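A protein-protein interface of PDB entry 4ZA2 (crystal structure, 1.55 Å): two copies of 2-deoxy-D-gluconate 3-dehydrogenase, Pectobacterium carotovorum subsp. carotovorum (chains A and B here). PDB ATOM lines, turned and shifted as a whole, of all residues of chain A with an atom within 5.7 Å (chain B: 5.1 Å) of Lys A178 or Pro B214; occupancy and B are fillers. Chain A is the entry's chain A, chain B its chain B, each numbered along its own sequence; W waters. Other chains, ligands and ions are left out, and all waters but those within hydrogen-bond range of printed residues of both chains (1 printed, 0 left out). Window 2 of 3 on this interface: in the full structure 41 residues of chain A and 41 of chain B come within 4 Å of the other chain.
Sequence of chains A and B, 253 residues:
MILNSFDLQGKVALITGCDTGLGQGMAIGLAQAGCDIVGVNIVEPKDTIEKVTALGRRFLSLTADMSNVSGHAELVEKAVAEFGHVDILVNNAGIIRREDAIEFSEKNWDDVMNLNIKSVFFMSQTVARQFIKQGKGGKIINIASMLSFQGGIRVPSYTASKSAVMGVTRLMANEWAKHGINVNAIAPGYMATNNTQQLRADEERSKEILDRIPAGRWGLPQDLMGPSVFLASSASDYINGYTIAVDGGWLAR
Printed residues of chain B that touch a printed residue of chain A: Pro B214, Ala B215 and Arg B253.
Printed residues of chain A that touch a printed residue of chain B: Ala A173, Asn A174, Ala A177 and Lys A178.
Of the printed residues of chain B, Ala A173 touches Pro B214.
Of the printed residues of chain B, Asn A174 touches Pro B214 (3.4 Å) and Arg B253 (3.3 Å).
Of the printed residues of chain B, Lys A178 touches Pro B214 (3.6 Å).
His A179 touches none of the printed residues of chain B.
Ile A181 touches none of the printed residues of chain B.
Of chain A, only Ala A173, Asn A174, Ala A177 and Lys A178 come within 4 Å of Pro B214.
Of the printed residues of chain A, Ala B215 touches Ala A177 (3.7 Å).
Printed residues of chain A within 4 Å of Arg B253: Asn A174.
The nearest printed residue of chain A that does not touch Ala B215 is Lys A178 (4.8 Å).
Water W1 lies within hydrogen-bond range of the backbone carbonyl oxygen of Asn A174, the backbone NH of Lys A178, the backbone carbonyl oxygen of Pro B214 and the backbone NH of Ala A177.
No position is printed for both chains.
Of the 6 pairs that touch across the chains among the printed residues, none has its exchanged pair printed and touching as well.
The backbone carbonyl oxygen (O) of Glu A175 is in hydrogen-bond range of the side-chain amino group (NZ) of Lys A178.
The backbone carbonyl oxygen of Gly B248 lies within hydrogen-bond range of the backbone NH of Ala B215, 2.9 Å away.
N of Arg B253 lies within hydrogen-bond range of OD1 of Asn A174, at 3.3 Å.
Among the printed residues, pairs that only touch across the chains: Asn A174 with Pro B214 (3.4 Å), Ala A177 with Pro B214 (3.5 Å), Lys A178 with Pro B214 (3.6 Å), Ala A177 with Ala B215 (3.7 Å) and Ala A173 with Pro B214 (3.7 Å).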
ATOM      1  N   ALA A 173      24.394  16.407  15.515  1.00  0.00           N
ATOM      2  CA  ALA A 173      24.049  15.902  16.844  1.00  0.00           C
ATOM      3  C   ALA A 173      23.022  16.802  17.554  1.00  0.00           C
ATOM      4  O   ALA A 173      22.017  16.326  18.082  1.00  0.00           O
ATOM      5  CB  ALA A 173      25.290  15.775  17.696  1.00  0.00           C
ATOM      6  N   ASN A 174      23.263  18.100  17.508  1.00  0.00           N
ATOM      7  CA  ASN A 174      22.398  19.086  18.179  1.00  0.00           C
ATOM      8  C   ASN A 174      20.966  18.938  17.751  1.00  0.00           C
ATOM      9  O   ASN A 174      20.063  18.999  18.589  1.00  0.00           O
ATOM     10  CB  ASN A 174      22.878  20.499  17.888  1.00  0.00           C
ATOM     11  CG  ASN A 174      24.179  20.826  18.599  1.00  0.00           C
ATOM     12  OD1 ASN A 174      24.547  20.179  19.574  1.00  0.00           O
ATOM     13  ND2 ASN A 174      24.878  21.844  18.112  1.00  0.00           N
ATOM     14  N   GLU A 175      20.764  18.733  16.452  1.00  0.00           N
ATOM     15  CA  GLU A 175      19.414  18.647  15.908  1.00  0.00           C
ATOM     16  C   GLU A 175      18.793  17.261  15.992  1.00  0.00           C
ATOM     17  O   GLU A 175      17.568  17.137  16.154  1.00  0.00           O
ATOM     18  CB  GLU A 175      19.375  19.135  14.469  1.00  0.00           C
ATOM     19  CG  GLU A 175      19.702  20.598  14.323  1.00  0.00           C
ATOM     20  CD  GLU A 175      19.273  21.185  12.992  1.00  0.00           C
ATOM     21  OE1 GLU A 175      20.048  21.983  12.429  1.00  0.00           O
ATOM     22  OE2 GLU A 175      18.157  20.892  12.524  1.00  0.00           O
ATOM     23  N   TRP A 176      19.599  16.214  15.847  1.00  0.00           N
ATOM     24  CA  TRP A 176      19.069  14.880  15.688  1.00  0.00           C
ATOM     25  C   TRP A 176      19.193  13.966  16.899  1.00  0.00           C
ATOM     26  O   TRP A 176      18.579  12.902  16.920  1.00  0.00           O
ATOM     27  CB  TRP A 176      19.709  14.228  14.452  1.00  0.00           C
ATOM     28  CG  TRP A 176      19.456  15.004  13.200  1.00  0.00           C
ATOM     29  CD1 TRP A 176      18.431  15.885  12.976  1.00  0.00           C
ATOM     30  CD2 TRP A 176      20.213  14.963  11.984  1.00  0.00           C
ATOM     31  NE1 TRP A 176      18.510  16.392  11.711  1.00  0.00           N
ATOM     32  CE2 TRP A 176      19.598  15.849  11.078  1.00  0.00           C
ATOM     33  CE3 TRP A 176      21.367  14.281  11.581  1.00  0.00           C
ATOM     34  CZ2 TRP A 176      20.088  16.064   9.789  1.00  0.00           C
ATOM     35  CZ3 TRP A 176      21.849  14.488  10.313  1.00  0.00           C
ATOM     36  CH2 TRP A 176      21.216  15.374   9.426  1.00  0.00           C
ATOM     37  N   ALA A 177      19.959  14.365  17.910  1.00  0.00           N
ATOM     38  CA  ALA A 177      20.118  13.540  19.120  1.00  0.00           C
ATOM     39  C   ALA A 177      18.782  13.202  19.773  1.00  0.00           C
ATOM     40  O   ALA A 177      18.615  12.112  20.330  1.00  0.00           O
ATOM     41  CB  ALA A 177      21.010  14.233  20.144  1.00  0.00           C
ATOM     42  N   LYS A 178      17.846  14.134  19.707  1.00  0.00           N
ATOM     43  CA  LYS A 178      16.500  13.916  20.263  1.00  0.00           C
ATOM     44  C   LYS A 178      15.782  12.721  19.659  1.00  0.00           C
ATOM     45  O   LYS A 178      14.865  12.167  20.278  1.00  0.00           O
ATOM     46  CB  LYS A 178      15.633  15.175  20.098  1.00  0.00           C
ATOM     47  CG  LYS A 178      15.162  15.474  18.673  1.00  0.00           C
ATOM     48  CD  LYS A 178      14.282  16.717  18.598  1.00  0.00           C
ATOM     49  CE  LYS A 178      15.083  18.017  18.614  1.00  0.00           C
ATOM     50  NZ  LYS A 178      15.575  18.442  17.267  1.00  0.00           N
ATOM     51  N   HIS A 179      16.184  12.310  18.457  1.00  0.00           N
ATOM     52  CA  HIS A 179      15.597  11.140  17.800  1.00  0.00           C
ATOM     53  C   HIS A 179      16.366   9.843  18.053  1.00  0.00           C
ATOM     54  O   HIS A 179      16.148   8.844  17.363  1.00  0.00           O
ATOM     55  CB  HIS A 179      15.502  11.357  16.288  1.00  0.00           C
ATOM     56  CG  HIS A 179      14.760  12.593  15.900  1.00  0.00           C
ATOM     57  ND1 HIS A 179      13.425  12.787  16.192  1.00  0.00           N
ATOM     58  CD2 HIS A 179      15.166  13.704  15.241  1.00  0.00           C
ATOM     59  CE1 HIS A 179      13.045  13.964  15.730  1.00  0.00           C
ATOM     60  NE2 HIS A 179      14.081  14.538  15.143  1.00  0.00           N
ATOM     61  N   GLY A 180      17.290   9.847  19.006  1.00  0.00           N
ATOM     62  CA  GLY A 180      18.128   8.679  19.234  1.00  0.00           C
ATOM     63  C   GLY A 180      19.131   8.452  18.105  1.00  0.00           C
ATOM     64  O   GLY A 180      19.575   7.324  17.857  1.00  0.00           O
ATOM     65  N   ILE A 181      19.478   9.534  17.420  1.00  0.00           N
ATOM     66  CA  ILE A 181      20.521   9.484  16.387  1.00  0.00           C
ATOM     67  C   ILE A 181      21.812  10.039  16.985  1.00  0.00           C
ATOM     68  O   ILE A 181      21.816  11.130  17.542  1.00  0.00           O
ATOM     69  CB  ILE A 181      20.143  10.283  15.126  1.00  0.00           C
ATOM     70  CG1 ILE A 181      18.882   9.682  14.495  1.00  0.00           C
ATOM     71  CG2 ILE A 181      21.299  10.294  14.129  1.00  0.00           C
ATOM     72  CD1 ILE A 181      18.213  10.547  13.438  1.00  0.00           C
ATOM     73  N   ARG B 212      19.813  22.383  26.919  1.00  0.00           N
ATOM     74  CA  ARG B 212      21.112  22.493  26.256  1.00  0.00           C
ATOM     75  C   ARG B 212      21.850  21.156  26.099  1.00  0.00           C
ATOM     76  O   ARG B 212      22.981  21.135  25.613  1.00  0.00           O
ATOM     77  CB  ARG B 212      21.988  23.475  27.027  1.00  0.00           C
ATOM     78  CG  ARG B 212      21.459  24.901  26.962  1.00  0.00           C
ATOM     79  CD  ARG B 212      22.145  25.783  27.986  1.00  0.00           C
ATOM     80  NE  ARG B 212      23.598  25.814  27.805  1.00  0.00           N
ATOM     81  CZ  ARG B 212      24.449  26.359  28.673  1.00  0.00           C
ATOM     82  NH1 ARG B 212      23.992  26.930  29.788  1.00  0.00           N
ATOM     83  NH2 ARG B 212      25.762  26.344  28.427  1.00  0.00           N
ATOM     84  N   ILE B 213      21.245  20.063  26.546  1.00  0.00           N
ATOM     85  CA  ILE B 213      21.751  18.720  26.244  1.00  0.00           C
ATOM     86  C   ILE B 213      20.985  18.173  25.030  1.00  0.00           C
ATOM     87  O   ILE B 213      19.790  17.863  25.128  1.00  0.00           O
ATOM     88  CB  ILE B 213      21.549  17.751  27.432  1.00  0.00           C
ATOM     89  CG1 ILE B 213      22.235  18.288  28.697  1.00  0.00           C
ATOM     90  CG2 ILE B 213      22.058  16.361  27.058  1.00  0.00           C
ATOM     91  CD1 ILE B 213      21.976  17.461  29.941  1.00  0.00           C
ATOM     92  N   PRO B 214      21.650  18.033  23.868  1.00  0.00           N
ATOM     93  CA  PRO B 214      20.950  17.532  22.687  1.00  0.00           C
ATOM     94  C   PRO B 214      20.192  16.216  22.900  1.00  0.00           C
ATOM     95  O   PRO B 214      19.065  16.089  22.419  1.00  0.00           O
ATOM     96  CB  PRO B 214      22.079  17.376  21.673  1.00  0.00           C
ATOM     97  CG  PRO B 214      22.995  18.498  22.023  1.00  0.00           C
ATOM     98  CD  PRO B 214      22.969  18.587  23.521  1.00  0.00           C
ATOM     99  N   ALA B 215      20.772  15.287  23.660  1.00  0.00           N
ATOM    100  CA  ALA B 215      20.128  14.011  23.955  1.00  0.00           C
ATOM    101  C   ALA B 215      18.836  14.177  24.753  1.00  0.00           C
ATOM    102  O   ALA B 215      18.019  13.268  24.780  1.00  0.00           O
ATOM    103  CB  ALA B 215      21.078  13.081  24.687  1.00  0.00           C
ATOM    104  N   GLY B 216      18.702  15.297  25.441  1.00  0.00           N
ATOM    105  CA  GLY B 216      17.448  15.612  26.169  1.00  0.00           C
ATOM    106  C   GLY B 216      17.221  14.746  27.395  1.00  0.00           C
ATOM    107  O   GLY B 216      16.066  14.529  27.798  1.00  0.00           O
ATOM    108  N   GLY B 248      26.013  13.461  25.965  1.00  0.00           N
ATOM    109  CA  GLY B 248      24.720  13.646  25.308  1.00  0.00           C
ATOM    110  C   GLY B 248      24.706  14.799  24.332  1.00  0.00           C
ATOM    111  O   GLY B 248      23.652  15.256  23.906  1.00  0.00           O
ATOM    112  N   GLY B 249      25.892  15.223  23.900  1.00  0.00           N
ATOM    113  CA  GLY B 249      26.015  16.378  23.001  1.00  0.00           C
ATOM    114  C   GLY B 249      26.262  17.730  23.644  1.00  0.00           C
ATOM    115  O   GLY B 249      26.260  18.741  22.944  1.00  0.00           O
ATOM    116  N   TRP B 250      26.488  17.769  24.954  1.00  0.00           N
ATOM    117  CA  TRP B 250      26.636  19.058  25.659  1.00  0.00           C
ATOM    118  C   TRP B 250      27.663  19.966  24.991  1.00  0.00           C
ATOM    119  O   TRP B 250      27.397  21.120  24.728  1.00  0.00           O
ATOM    120  CB  TRP B 250      27.037  18.858  27.112  1.00  0.00           C
ATOM    121  CG  TRP B 250      27.301  20.132  27.837  1.00  0.00           C
ATOM    122  CD1 TRP B 250      28.519  20.771  27.975  1.00  0.00           C
ATOM    123  CD2 TRP B 250      26.340  20.963  28.509  1.00  0.00           C
ATOM    124  NE1 TRP B 250      28.367  21.925  28.711  1.00  0.00           N
ATOM    125  CE2 TRP B 250      27.042  22.067  29.043  1.00  0.00           C
ATOM    126  CE3 TRP B 250      24.952  20.878  28.712  1.00  0.00           C
ATOM    127  CZ2 TRP B 250      26.403  23.080  29.772  1.00  0.00           C
ATOM    128  CZ3 TRP B 250      24.325  21.894  29.444  1.00  0.00           C
ATOM    129  CH2 TRP B 250      25.055  22.974  29.950  1.00  0.00           C
ATOM    130  N   ARG B 253      26.712  21.716  21.587  1.00  0.00           N
ATOM    131  CA  ARG B 253      25.650  22.706  21.522  1.00  0.00           C
ATOM    132  C   ARG B 253      26.210  24.131  21.556  1.00  0.00           C
ATOM    133  O   ARG B 253      26.877  24.529  22.518  1.00  0.00           O
ATOM    134  CB  ARG B 253      24.655  22.443  22.656  1.00  0.00           C
ATOM    135  CG  ARG B 253      23.320  23.157  22.530  1.00  0.00           C
ATOM    136  CD  ARG B 253      22.589  22.849  21.239  1.00  0.00           C
ATOM    137  NE  ARG B 253      21.421  23.721  21.074  1.00  0.00           N
ATOM    138  CZ  ARG B 253      21.420  24.901  20.461  1.00  0.00           C
ATOM    139  NH1 ARG B 253      22.532  25.405  19.918  1.00  0.00           N
ATOM    140  NH2 ARG B 253      20.284  25.590  20.378  1.00  0.00           N
HETATM  141  O   HOH W   1      18.533  16.938  19.636  1.00  0.00           O
